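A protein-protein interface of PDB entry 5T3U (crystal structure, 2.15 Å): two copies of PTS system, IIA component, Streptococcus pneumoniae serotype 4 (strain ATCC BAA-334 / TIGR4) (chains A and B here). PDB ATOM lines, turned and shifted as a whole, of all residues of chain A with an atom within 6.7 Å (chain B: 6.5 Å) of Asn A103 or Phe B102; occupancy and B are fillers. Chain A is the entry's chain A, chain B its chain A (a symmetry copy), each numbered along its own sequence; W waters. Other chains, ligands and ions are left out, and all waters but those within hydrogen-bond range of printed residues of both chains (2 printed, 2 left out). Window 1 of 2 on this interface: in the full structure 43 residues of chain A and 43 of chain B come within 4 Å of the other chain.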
ATOM      1  N   PHE A  19      21.471 -28.935  27.188  1.00  0.00           N
ATOM      2  CA  PHE A  19      21.001 -27.677  27.827  1.00  0.00           C
ATOM      3  C   PHE A  19      21.440 -27.529  29.290  1.00  0.00           C
ATOM      4  O   PHE A  19      21.987 -26.471  29.677  1.00  0.00           O
ATOM      5  CB  PHE A  19      19.476 -27.552  27.745  1.00  0.00           C
ATOM      6  CG  PHE A  19      18.928 -26.205  28.180  1.00  0.00           C
ATOM      7  CD1 PHE A  19      19.319 -25.032  27.541  1.00  0.00           C
ATOM      8  CD2 PHE A  19      17.981 -26.123  29.201  1.00  0.00           C
ATOM      9  CE1 PHE A  19      18.782 -23.819  27.900  1.00  0.00           C
ATOM     10  CE2 PHE A  19      17.458 -24.913  29.579  1.00  0.00           C
ATOM     11  CZ  PHE A  19      17.880 -23.736  28.919  1.00  0.00           C
ATOM     12  N   ALA A  23      24.110 -24.992  30.774  1.00  0.00           N
ATOM     13  CA  ALA A  23      23.640 -24.005  31.763  1.00  0.00           C
ATOM     14  C   ALA A  23      24.495 -23.966  33.035  1.00  0.00           C
ATOM     15  O   ALA A  23      24.832 -22.892  33.524  1.00  0.00           O
ATOM     16  CB  ALA A  23      22.172 -24.221  32.106  1.00  0.00           C
ATOM     17  N   LEU A  74      15.470 -28.379  38.326  1.00  0.00           N
ATOM     18  CA  LEU A  74      15.194 -27.475  37.195  1.00  0.00           C
ATOM     19  C   LEU A  74      15.094 -28.320  35.946  1.00  0.00           C
ATOM     20  O   LEU A  74      15.996 -29.120  35.658  1.00  0.00           O
ATOM     21  CB  LEU A  74      16.303 -26.441  37.037  1.00  0.00           C
ATOM     22  CG  LEU A  74      16.580 -25.525  38.237  1.00  0.00           C
ATOM     23  CD1 LEU A  74      17.684 -24.516  37.851  1.00  0.00           C
ATOM     24  CD2 LEU A  74      15.316 -24.820  38.761  1.00  0.00           C
ATOM     25  N   THR A 100      10.123 -25.655  35.988  1.00  0.00           N
ATOM     26  CA  THR A 100      10.429 -25.946  34.601  1.00  0.00           C
ATOM     27  C   THR A 100      10.694 -24.660  33.782  1.00  0.00           C
ATOM     28  O   THR A 100      10.493 -23.562  34.286  1.00  0.00           O
ATOM     29  CB  THR A 100       9.360 -26.856  33.914  1.00  0.00           C
ATOM     30  OG1 THR A 100       9.884 -27.297  32.660  1.00  0.00           O
ATOM     31  CG2 THR A 100       8.096 -26.107  33.640  1.00  0.00           C
ATOM     32  N   GLY A 101      11.155 -24.808  32.541  1.00  0.00           N
ATOM     33  CA  GLY A 101      11.398 -23.631  31.688  1.00  0.00           C
ATOM     34  C   GLY A 101      12.506 -22.710  32.189  1.00  0.00           C
ATOM     35  O   GLY A 101      12.505 -21.506  31.875  1.00  0.00           O
ATOM     36  N   PHE A 102      13.474 -23.262  32.935  1.00  0.00           N
ATOM     37  CA  PHE A 102      14.514 -22.449  33.570  1.00  0.00           C
ATOM     38  C   PHE A 102      15.409 -21.680  32.593  1.00  0.00           C
ATOM     39  O   PHE A 102      15.615 -22.103  31.442  1.00  0.00           O
ATOM     40  CB  PHE A 102      15.397 -23.294  34.521  1.00  0.00           C
ATOM     41  CG  PHE A 102      16.447 -24.143  33.830  1.00  0.00           C
ATOM     42  CD1 PHE A 102      16.174 -25.461  33.465  1.00  0.00           C
ATOM     43  CD2 PHE A 102      17.721 -23.645  33.599  1.00  0.00           C
ATOM     44  CE1 PHE A 102      17.162 -26.266  32.828  1.00  0.00           C
ATOM     45  CE2 PHE A 102      18.699 -24.423  32.965  1.00  0.00           C
ATOM     46  CZ  PHE A 102      18.418 -25.744  32.586  1.00  0.00           C
ATOM     47  N   ASN A 103      15.985 -20.593  33.090  1.00  0.00           N
ATOM     48  CA  ASN A 103      16.929 -19.788  32.334  1.00  0.00           C
ATOM     49  C   ASN A 103      18.189 -19.561  33.187  1.00  0.00           C
ATOM     50  O   ASN A 103      18.284 -20.060  34.306  1.00  0.00           O
ATOM     51  CB  ASN A 103      16.270 -18.471  31.859  1.00  0.00           C
ATOM     52  CG  ASN A 103      15.706 -17.652  32.996  1.00  0.00           C
ATOM     53  OD1 ASN A 103      15.912 -17.990  34.171  1.00  0.00           O
ATOM     54  ND2 ASN A 103      14.992 -16.559  32.667  1.00  0.00           N
ATOM     55  N   ILE A 104      19.184 -18.866  32.645  1.00  0.00           N
ATOM     56  CA  ILE A 104      20.425 -18.654  33.398  1.00  0.00           C
ATOM     57  C   ILE A 104      20.152 -17.836  34.673  1.00  0.00           C
ATOM     58  O   ILE A 104      20.621 -18.195  35.735  1.00  0.00           O
ATOM     59  CB  ILE A 104      21.550 -18.086  32.487  1.00  0.00           C
ATOM     60  CG1 ILE A 104      22.220 -19.235  31.751  1.00  0.00           C
ATOM     61  CG2 ILE A 104      22.617 -17.223  33.270  1.00  0.00           C
ATOM     62  CD1 ILE A 104      23.029 -20.186  32.623  1.00  0.00           C
ATOM     63  N   PRO A 105      19.335 -16.768  34.589  1.00  0.00           N
ATOM     64  CA  PRO A 105      19.057 -16.010  35.831  1.00  0.00           C
ATOM     65  C   PRO A 105      18.499 -16.835  37.008  1.00  0.00           C
ATOM     66  O   PRO A 105      18.925 -16.611  38.151  1.00  0.00           O
ATOM     67  CB  PRO A 105      18.028 -14.980  35.375  1.00  0.00           C
ATOM     68  CG  PRO A 105      18.422 -14.708  33.924  1.00  0.00           C
ATOM     69  CD  PRO A 105      18.759 -16.085  33.405  1.00  0.00           C
ATOM     70  N   LEU A 106      17.558 -17.753  36.749  1.00  0.00           N
ATOM     71  CA  LEU A 106      17.085 -18.679  37.784  1.00  0.00           C
ATOM     72  C   LEU A 106      18.219 -19.533  38.358  1.00  0.00           C
ATOM     73  O   LEU A 106      18.402 -19.601  39.591  1.00  0.00           O
ATOM     74  CB  LEU A 106      15.976 -19.595  37.241  1.00  0.00           C
ATOM     75  CG  LEU A 106      15.273 -20.528  38.285  1.00  0.00           C
ATOM     76  CD1 LEU A 106      14.704 -19.798  39.492  1.00  0.00           C
ATOM     77  CD2 LEU A 106      14.157 -21.310  37.597  1.00  0.00           C
ATOM     78  N   LEU A 107      18.991 -20.183  37.476  1.00  0.00           N
ATOM     79  CA  LEU A 107      20.051 -21.093  37.927  1.00  0.00           C
ATOM     80  C   LEU A 107      21.085 -20.339  38.764  1.00  0.00           C
ATOM     81  O   LEU A 107      21.402 -20.749  39.878  1.00  0.00           O
ATOM     82  CB  LEU A 107      20.706 -21.862  36.755  1.00  0.00           C
ATOM     83  CG  LEU A 107      21.832 -22.846  37.176  1.00  0.00           C
ATOM     84  CD1 LEU A 107      21.387 -23.837  38.301  1.00  0.00           C
ATOM     85  CD2 LEU A 107      22.417 -23.606  35.956  1.00  0.00           C
ATOM     86  N   VAL A 108      21.578 -19.211  38.250  1.00  0.00           N
ATOM     87  CA  VAL A 108      22.499 -18.359  38.999  1.00  0.00           C
ATOM     88  C   VAL A 108      21.986 -17.963  40.379  1.00  0.00           C
ATOM     89  O   VAL A 108      22.722 -18.055  41.354  1.00  0.00           O
ATOM     90  CB  VAL A 108      22.860 -17.069  38.196  1.00  0.00           C
ATOM     91  CG1 VAL A 108      23.607 -16.058  39.111  1.00  0.00           C
ATOM     92  CG2 VAL A 108      23.704 -17.445  36.994  1.00  0.00           C
ATOM     93  N   ASN A 126      10.998 -13.397  39.770  1.00  0.00           N
ATOM     94  CA  ASN A 126      12.086 -12.579  39.238  1.00  0.00           C
ATOM     95  C   ASN A 126      12.757 -13.203  37.991  1.00  0.00           C
ATOM     96  O   ASN A 126      13.201 -12.483  37.097  1.00  0.00           O
ATOM     97  CB  ASN A 126      13.151 -12.308  40.303  1.00  0.00           C
ATOM     98  CG  ASN A 126      12.676 -11.372  41.426  1.00  0.00           C
ATOM     99  OD1 ASN A 126      11.672 -10.655  41.323  1.00  0.00           O
ATOM    100  ND2 ASN A 126      13.448 -11.350  42.493  1.00  0.00           N
ATOM    101  N   ALA A 127      12.841 -14.526  37.957  1.00  0.00           N
ATOM    102  CA  ALA A 127      13.405 -15.238  36.813  1.00  0.00           C
ATOM    103  C   ALA A 127      12.532 -15.094  35.564  1.00  0.00           C
ATOM    104  O   ALA A 127      13.081 -14.977  34.457  1.00  0.00           O
ATOM    105  CB  ALA A 127      13.606 -16.709  37.138  1.00  0.00           C
ATOM    106  N   GLN A 128      11.202 -15.121  35.735  1.00  0.00           N
ATOM    107  CA  GLN A 128      10.264 -14.816  34.630  1.00  0.00           C
ATOM    108  C   GLN A 128      10.491 -13.400  34.082  1.00  0.00           C
ATOM    109  O   GLN A 128      10.540 -13.204  32.878  1.00  0.00           O
ATOM    110  CB  GLN A 128       8.788 -14.962  35.053  1.00  0.00           C
ATOM    111  CG  GLN A 128       8.391 -16.391  35.439  1.00  0.00           C
ATOM    112  CD  GLN A 128       7.014 -16.461  36.068  1.00  0.00           C
ATOM    113  OE1 GLN A 128       6.559 -15.491  36.687  1.00  0.00           O
ATOM    114  NE2 GLN A 128       6.347 -17.619  35.935  1.00  0.00           N
ATOM    115  N   ASN A 129      10.665 -12.436  34.981  1.00  0.00           N
ATOM    116  CA  ASN A 129      10.865 -11.053  34.604  1.00  0.00           C
ATOM    117  C   ASN A 129      12.229 -10.812  34.003  1.00  0.00           C
ATOM    118  O   ASN A 129      12.436  -9.769  33.411  1.00  0.00           O
ATOM    119  CB  ASN A 129      10.698 -10.132  35.818  1.00  0.00           C
ATOM    120  CG  ASN A 129       9.222  -9.879  36.184  1.00  0.00           C
ATOM    121  OD1 ASN A 129       8.308 -10.093  35.377  1.00  0.00           O
ATOM    122  ND2 ASN A 129       8.999  -9.404  37.410  1.00  0.00           N
ATOM    123  N   SER A 130      13.171 -11.744  34.222  1.00  0.00           N
ATOM    124  CA  SER A 130      14.504 -11.691  33.605  1.00  0.00           C
ATOM    125  C   SER A 130      14.549 -12.132  32.129  1.00  0.00           C
ATOM    126  O   SER A 130      15.567 -11.951  31.456  1.00  0.00           O
ATOM    127  CB  SER A 130      15.468 -12.553  34.373  1.00  0.00           C
ATOM    128  OG  SER A 130      15.717 -12.008  35.660  1.00  0.00           O
ATOM    129  N   LEU A 131      13.474 -12.739  31.652  1.00  0.00           N
ATOM    130  CA  LEU A 131      13.303 -13.032  30.240  1.00  0.00           C
ATOM    131  C   LEU A 131      12.500 -11.886  29.613  1.00  0.00           C
ATOM    132  O   LEU A 131      11.304 -11.740  29.890  1.00  0.00           O
ATOM    133  CB  LEU A 131      12.571 -14.360  30.060  1.00  0.00           C
ATOM    134  CG  LEU A 131      12.554 -15.002  28.655  1.00  0.00           C
ATOM    135  CD1 LEU A 131      12.092 -16.468  28.735  1.00  0.00           C
ATOM    136  CD2 LEU A 131      11.675 -14.219  27.676  1.00  0.00           C
ATOM    137  N   PHE A 132      13.151 -11.058  28.790  1.00  0.00           N
ATOM    138  CA  PHE A 132      12.452  -9.925  28.228  1.00  0.00           C
ATOM    139  C   PHE A 132      13.084  -9.344  26.967  1.00  0.00           C
ATOM    140  O   PHE A 132      14.270  -9.503  26.726  1.00  0.00           O
ATOM    141  CB  PHE A 132      12.277  -8.800  29.287  1.00  0.00           C
ATOM    142  CG  PHE A 132      13.583  -8.205  29.788  1.00  0.00           C
ATOM    143  CD1 PHE A 132      14.253  -8.778  30.872  1.00  0.00           C
ATOM    144  CD2 PHE A 132      14.116  -7.054  29.198  1.00  0.00           C
ATOM    145  CE1 PHE A 132      15.451  -8.193  31.376  1.00  0.00           C
ATOM    146  CE2 PHE A 132      15.294  -6.477  29.679  1.00  0.00           C
ATOM    147  CZ  PHE A 132      15.971  -7.047  30.770  1.00  0.00           C
ATOM    148  N   VAL B  13      21.960 -17.224  18.984  1.00  0.00           N
ATOM    149  CA  VAL B  13      21.843 -17.520  20.413  1.00  0.00           C
ATOM    150  C   VAL B  13      23.218 -17.270  20.974  1.00  0.00           C
ATOM    151  O   VAL B  13      24.187 -17.939  20.560  1.00  0.00           O
ATOM    152  CB  VAL B  13      21.503 -19.006  20.689  1.00  0.00           C
ATOM    153  CG1 VAL B  13      21.099 -19.201  22.122  1.00  0.00           C
ATOM    154  CG2 VAL B  13      20.409 -19.509  19.767  1.00  0.00           C
ATOM    155  N   ALA B  14      23.323 -16.336  21.916  1.00  0.00           N
ATOM    156  CA  ALA B  14      24.646 -15.957  22.429  1.00  0.00           C
ATOM    157  C   ALA B  14      24.707 -15.968  23.948  1.00  0.00           C
ATOM    158  O   ALA B  14      23.771 -15.565  24.590  1.00  0.00           O
ATOM    159  CB  ALA B  14      25.027 -14.577  21.910  1.00  0.00           C
ATOM    160  N   SER B  15      25.828 -16.406  24.526  1.00  0.00           N
ATOM    161  CA  SER B  15      25.951 -16.415  25.975  1.00  0.00           C
ATOM    162  C   SER B  15      27.417 -16.412  26.388  1.00  0.00           C
ATOM    163  O   SER B  15      28.301 -16.724  25.581  1.00  0.00           O
ATOM    164  CB  SER B  15      25.300 -17.700  26.522  1.00  0.00           C
ATOM    165  OG  SER B  15      26.054 -18.821  26.107  1.00  0.00           O
ATOM    166  N   PHE B  19      26.141 -22.275  27.412  1.00  0.00           N
ATOM    167  CA  PHE B  19      24.658 -22.187  27.475  1.00  0.00           C
ATOM    168  C   PHE B  19      23.983 -22.172  26.097  1.00  0.00           C
ATOM    169  O   PHE B  19      23.036 -22.955  25.854  1.00  0.00           O
ATOM    170  CB  PHE B  19      24.211 -20.953  28.267  1.00  0.00           C
ATOM    171  CG  PHE B  19      22.724 -20.897  28.563  1.00  0.00           C
ATOM    172  CD1 PHE B  19      22.099 -21.910  29.286  1.00  0.00           C
ATOM    173  CD2 PHE B  19      21.962 -19.802  28.156  1.00  0.00           C
ATOM    174  CE1 PHE B  19      20.763 -21.832  29.600  1.00  0.00           C
ATOM    175  CE2 PHE B  19      20.624 -19.729  28.447  1.00  0.00           C
ATOM    176  CZ  PHE B  19      20.013 -20.776  29.175  1.00  0.00           C
ATOM    177  N   ALA B  20      24.476 -21.283  25.214  1.00  0.00           N
ATOM    178  CA  ALA B  20      23.956 -21.099  23.861  1.00  0.00           C
ATOM    179  C   ALA B  20      24.041 -22.327  22.975  1.00  0.00           C
ATOM    180  O   ALA B  20      23.031 -22.729  22.393  1.00  0.00           O
ATOM    181  CB  ALA B  20      24.662 -19.877  23.163  1.00  0.00           C
ATOM    182  N   ALA B  23      21.797 -25.044  24.439  1.00  0.00           N
ATOM    183  CA  ALA B  23      20.390 -24.736  24.125  1.00  0.00           C
ATOM    184  C   ALA B  23      19.998 -25.094  22.686  1.00  0.00           C
ATOM    185  O   ALA B  23      18.939 -25.671  22.457  1.00  0.00           O
ATOM    186  CB  ALA B  23      20.059 -23.281  24.429  1.00  0.00           C
ATOM    187  N   LEU B  24      20.857 -24.810  21.720  1.00  0.00           N
ATOM    188  CA  LEU B  24      20.510 -25.154  20.334  1.00  0.00           C
ATOM    189  C   LEU B  24      20.429 -26.647  20.140  1.00  0.00           C
ATOM    190  O   LEU B  24      19.501 -27.115  19.523  1.00  0.00           O
ATOM    191  CB  LEU B  24      21.501 -24.584  19.313  1.00  0.00           C
ATOM    192  CG  LEU B  24      21.130 -24.859  17.835  1.00  0.00           C
ATOM    193  CD1 LEU B  24      19.671 -24.407  17.430  1.00  0.00           C
ATOM    194  CD2 LEU B  24      22.166 -24.204  16.901  1.00  0.00           C
ATOM    195  N   LEU B  74      19.191 -13.906  20.930  1.00  0.00           N
ATOM    196  CA  LEU B  74      18.853 -14.387  22.282  1.00  0.00           C
ATOM    197  C   LEU B  74      20.114 -14.342  23.114  1.00  0.00           C
ATOM    198  O   LEU B  74      21.153 -14.879  22.703  1.00  0.00           O
ATOM    199  CB  LEU B  74      18.308 -15.810  22.236  1.00  0.00           C
ATOM    200  CG  LEU B  74      17.053 -16.051  21.388  1.00  0.00           C
ATOM    201  CD1 LEU B  74      16.631 -17.529  21.529  1.00  0.00           C
ATOM    202  CD2 LEU B  74      15.900 -15.091  21.734  1.00  0.00           C
ATOM    203  N   THR B  75      20.048 -13.669  24.260  1.00  0.00           N
ATOM    204  CA  THR B  75      21.207 -13.632  25.151  1.00  0.00           C
ATOM    205  C   THR B  75      20.852 -14.208  26.537  1.00  0.00           C
ATOM    206  O   THR B  75      19.683 -14.248  26.935  1.00  0.00           O
ATOM    207  CB  THR B  75      21.758 -12.213  25.318  1.00  0.00           C
ATOM    208  OG1 THR B  75      20.772 -11.434  25.988  1.00  0.00           O
ATOM    209  CG2 THR B  75      22.123 -11.573  23.918  1.00  0.00           C
ATOM    210  N   ASP B  76      21.883 -14.652  27.247  1.00  0.00           N
ATOM    211  CA  ASP B  76      21.689 -15.416  28.471  1.00  0.00           C
ATOM    212  C   ASP B  76      21.119 -14.601  29.626  1.00  0.00           C
ATOM    213  O   ASP B  76      20.223 -15.070  30.316  1.00  0.00           O
ATOM    214  CB  ASP B  76      22.964 -16.195  28.873  1.00  0.00           C
ATOM    215  CG  ASP B  76      24.248 -15.339  28.864  1.00  0.00           C
ATOM    216  OD1 ASP B  76      24.237 -14.171  28.395  1.00  0.00           O
ATOM    217  OD2 ASP B  76      25.301 -15.886  29.303  1.00  0.00           O
ATOM    218  N   LEU B  77      21.622 -13.380  29.812  1.00  0.00           N
ATOM    219  CA  LEU B  77      21.112 -12.520  30.858  1.00  0.00           C
ATOM    220  C   LEU B  77      21.447 -11.025  30.619  1.00  0.00           C
ATOM    221  O   LEU B  77      22.434 -10.699  29.947  1.00  0.00           O
ATOM    222  CB  LEU B  77      21.626 -13.008  32.222  1.00  0.00           C
ATOM    223  CG  LEU B  77      23.032 -12.673  32.696  1.00  0.00           C
ATOM    224  CD1 LEU B  77      23.285 -13.320  34.072  1.00  0.00           C
ATOM    225  CD2 LEU B  77      24.138 -13.080  31.718  1.00  0.00           C
ATOM    226  N   VAL B  99      16.374 -10.390  22.802  1.00  0.00           N
ATOM    227  CA  VAL B  99      15.577 -10.908  23.930  1.00  0.00           C
ATOM    228  C   VAL B  99      16.543 -11.601  24.878  1.00  0.00           C
ATOM    229  O   VAL B  99      17.276 -12.505  24.476  1.00  0.00           O
ATOM    230  CB  VAL B  99      14.427 -11.856  23.480  1.00  0.00           C
ATOM    231  CG1 VAL B  99      13.599 -12.342  24.679  1.00  0.00           C
ATOM    232  CG2 VAL B  99      13.503 -11.145  22.501  1.00  0.00           C
ATOM    233  N   THR B 100      16.579 -11.145  26.129  1.00  0.00           N
ATOM    234  CA  THR B 100      17.526 -11.718  27.066  1.00  0.00           C
ATOM    235  C   THR B 100      16.854 -12.722  28.031  1.00  0.00           C
ATOM    236  O   THR B 100      15.635 -12.842  28.038  1.00  0.00           O
ATOM    237  CB  THR B 100      18.353 -10.639  27.840  1.00  0.00           C
ATOM    238  OG1 THR B 100      19.423 -11.297  28.521  1.00  0.00           O
ATOM    239  CG2 THR B 100      17.520  -9.944  28.868  1.00  0.00           C
ATOM    240  N   GLY B 101      17.651 -13.441  28.820  1.00  0.00           N
ATOM    241  CA  GLY B 101      17.082 -14.394  29.790  1.00  0.00           C
ATOM    242  C   GLY B 101      16.339 -15.567  29.158  1.00  0.00           C
ATOM    243  O   GLY B 101      15.445 -16.154  29.794  1.00  0.00           O
ATOM    244  N   PHE B 102      16.718 -15.942  27.927  1.00  0.00           N
ATOM    245  CA  PHE B 102      15.992 -16.972  27.180  1.00  0.00           C
ATOM    246  C   PHE B 102      15.990 -18.356  27.836  1.00  0.00           C
ATOM    247  O   PHE B 102      16.920 -18.716  28.579  1.00  0.00           O
ATOM    248  CB  PHE B 102      16.509 -17.092  25.725  1.00  0.00           C
ATOM    249  CG  PHE B 102      17.807 -17.861  25.572  1.00  0.00           C
ATOM    250  CD1 PHE B 102      19.037 -17.202  25.593  1.00  0.00           C
ATOM    251  CD2 PHE B 102      17.798 -19.231  25.349  1.00  0.00           C
ATOM    252  CE1 PHE B 102      20.257 -17.919  25.437  1.00  0.00           C
ATOM    253  CE2 PHE B 102      18.992 -19.950  25.202  1.00  0.00           C
ATOM    254  CZ  PHE B 102      20.227 -19.286  25.238  1.00  0.00           C
ATOM    255  N   ASN B 103      14.975 -19.141  27.496  1.00  0.00           N
ATOM    256  CA  ASN B 103      14.855 -20.514  27.956  1.00  0.00           C
ATOM    257  C   ASN B 103      14.589 -21.426  26.746  1.00  0.00           C
ATOM    258  O   ASN B 103      14.539 -20.957  25.611  1.00  0.00           O
ATOM    259  CB  ASN B 103      13.773 -20.632  29.057  1.00  0.00           C
ATOM    260  CG  ASN B 103      12.421 -20.130  28.609  1.00  0.00           C
ATOM    261  OD1 ASN B 103      12.236 -19.806  27.426  1.00  0.00           O
ATOM    262  ND2 ASN B 103      11.453 -20.063  29.543  1.00  0.00           N
ATOM    263  N   ILE B 104      14.480 -22.731  26.969  1.00  0.00           N
ATOM    264  CA  ILE B 104      14.266 -23.651  25.847  1.00  0.00           C
ATOM    265  C   ILE B 104      12.925 -23.356  25.153  1.00  0.00           C
ATOM    266  O   ILE B 104      12.873 -23.286  23.941  1.00  0.00           O
ATOM    267  CB  ILE B 104      14.464 -25.131  26.283  1.00  0.00           C
ATOM    268  CG1 ILE B 104      15.946 -25.465  26.244  1.00  0.00           C
ATOM    269  CG2 ILE B 104      13.635 -26.158  25.414  1.00  0.00           C
ATOM    270  CD1 ILE B 104      16.572 -25.503  24.856  1.00  0.00           C
ATOM    271  N   LEU B 106      11.282 -20.520  24.600  1.00  0.00           N
ATOM    272  CA  LEU B 106      11.498 -19.417  23.657  1.00  0.00           C
ATOM    273  C   LEU B 106      12.254 -19.865  22.403  1.00  0.00           C
ATOM    274  O   LEU B 106      11.805 -19.614  21.266  1.00  0.00           O
ATOM    275  CB  LEU B 106      12.254 -18.258  24.327  1.00  0.00           C
ATOM    276  CG  LEU B 106      12.415 -16.951  23.478  1.00  0.00           C
ATOM    277  CD1 LEU B 106      11.107 -16.387  22.946  1.00  0.00           C
ATOM    278  CD2 LEU B 106      13.120 -15.886  24.314  1.00  0.00           C
ATOM    279  N   LEU B 107      13.399 -20.536  22.597  1.00  0.00           N
ATOM    280  CA  LEU B 107      14.240 -20.937  21.462  1.00  0.00           C
ATOM    281  C   LEU B 107      13.472 -21.874  20.529  1.00  0.00           C
ATOM    282  O   LEU B 107      13.403 -21.635  19.326  1.00  0.00           O
ATOM    283  CB  LEU B 107      15.588 -21.548  21.914  1.00  0.00           C
ATOM    284  CG  LEU B 107      16.522 -21.984  20.752  1.00  0.00           C
ATOM    285  CD1 LEU B 107      16.759 -20.850  19.702  1.00  0.00           C
ATOM    286  CD2 LEU B 107      17.866 -22.553  21.278  1.00  0.00           C
ATOM    287  N   LEU B 131       8.252 -20.630  32.254  1.00  0.00           N
ATOM    288  CA  LEU B 131       9.094 -20.801  33.425  1.00  0.00           C
ATOM    289  C   LEU B 131       8.193 -20.771  34.665  1.00  0.00           C
ATOM    290  O   LEU B 131       7.647 -19.718  35.014  1.00  0.00           O
ATOM    291  CB  LEU B 131      10.135 -19.685  33.494  1.00  0.00           C
ATOM    292  CG  LEU B 131      11.312 -19.843  34.481  1.00  0.00           C
ATOM    293  CD1 LEU B 131      12.422 -18.824  34.169  1.00  0.00           C
ATOM    294  CD2 LEU B 131      10.862 -19.710  35.939  1.00  0.00           C
HETATM  295  O   HOH W   1      18.882 -17.379  30.258  1.00  0.00           O
HETATM  296  O   HOH W   2      14.197 -23.816  29.566  1.00  0.00           O
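Phe B102 touches just one residue of chain A: Asn A103. Printed residues of chain B within 4 Å of Leu A131: Thr B100 (3.2 Å), Gly B101 (3.3 Å) and Asn B103 (3.6 Å). Printed residues of chain B within 4 Å of Phe A19: Phe B19 (3.3 Å), Ala B23 (3.6 Å) and Ile B104 (3.6 Å). Of the printed residues of chain A, Leu B131 touches Thr A100 (3.2 Å), Gly A101 (3.3 Å), Asn A103 (3.6 Å), Ala A127 (3.8 Å) and Gln A128 (2.6 Å). Printed residues of chain B within 4 Å of Ile A104: Phe B19 (3.6 Å) and Asp B76 (3.9 Å). Val A108 touches none of the printed residues of chain B. The nearest residue of chain A that does not touch Phe B102 is Leu A131 (4.2 Å). The nearest printed residue of chain A that does not touch Leu B131 is Leu A106 (4.02 Å).
Water W1 lies within hydrogen-bond range of O of Asp B76 (2.7 Å), N of Ile A104 (2.8 Å) and O of Phe B102 (2.9 Å). Water W2 bridges N of Ile B104 (2.8 Å) and O of Phe A102 (2.9 Å).
Phe A19 touches its own counterpart, Phe B19. Gly A101 touches Asn B103, and with the chains exchanged Asn A103 touches Gly B101. Phe A102 touches Asn B103, and with the chains exchanged Asn A103 touches Phe B102. Asn A103 touches Leu B131, and with the chains exchanged Leu A131 touches Asn B103. Positions printed for both chains: 19, 23, 74, 100, 101, 102, 103, 104, 106, 107 and 131. Of the 23 pairs that touch across the chains among the printed residues, 15 have their exchanged pair printed and touching as well.
The backbone carbonyl oxygen (O) of Phe A132 lies within hydrogen-bond range of the backbone NH (N) of Thr B100. The side-chain amide nitrogen (NE2) of Gln A128 lies within hydrogen-bond range of the backbone carbonyl oxygen (O) of Leu B131 (2.6 Å). The backbone carbonyl oxygen (O) of Gly A101 is in hydrogen-bond range of the side-chain amide nitrogen (ND2) of Asn B103 (2.9 Å). The side-chain amide nitrogen (ND2) of Asn A103 lies within hydrogen-bond range of the backbone carbonyl oxygen (O) of Gly B101 (2.9 Å).
O of Asp B76 sits close to N of Gly B101, at 3.4 Å. The side-chain amide oxygen (OD1) of Asn B103 sits at hydrogen-bond distance from the backbone NH (N) of Leu B106. The backbone NH (N) of Leu B77 sits close to the side-chain hydroxyl (OG1) of Thr B100. The backbone carbonyl oxygen (O) of Ala A127 sits at hydrogen-bond distance from the side-chain amide nitrogen (ND2) of Asn A103 (3.1 Å). The side-chain amide oxygen of Asn A103 is in hydrogen-bond range of the backbone NH of Leu A106, 3.1 Å away. OG1 of Thr B75 is in hydrogen-bond range of OG1 of Thr B100 (2.9 Å).
Ile B104 touches Phe A19 (CG1 to CG, 3.6 Å). CA of Ala A23 touches CD1 of Phe B19, 3.6 Å away. Thr A100 touches Leu B131 (O to CA, 3.2 Å). Leu B131 touches Gly A101 (CG to O, 3.3 Å). Phe A102 touches Asn B103 (O to CB, 3.4 Å). Asn A103 touches Leu B131 (OD1 to CD1, 3.6 Å). Ile A104 touches Asp B76 (CB to O, 3.9 Å). Ala A127 touches Leu B131. O of Ser A130 touches O of Thr B100, 3.5 Å away. O of Phe A132 touches CA of Val B99 (3.4 Å).
Printed residues of chain A that touch a printed residue of chain B: Phe A19, Ala A23, Thr A100, Gly A101, Phe A102, Asn A103, Ile A104, Pro A105, Ala A127, Gln A128, Ser A130, Leu A131 and Phe A132. Hydrophobic or aromatic side chains of chain A that line the printed part of chain B: Phe A19, Ala A23, Ile A104, Pro A105, Ala A127, Leu A131 and Phe A132.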
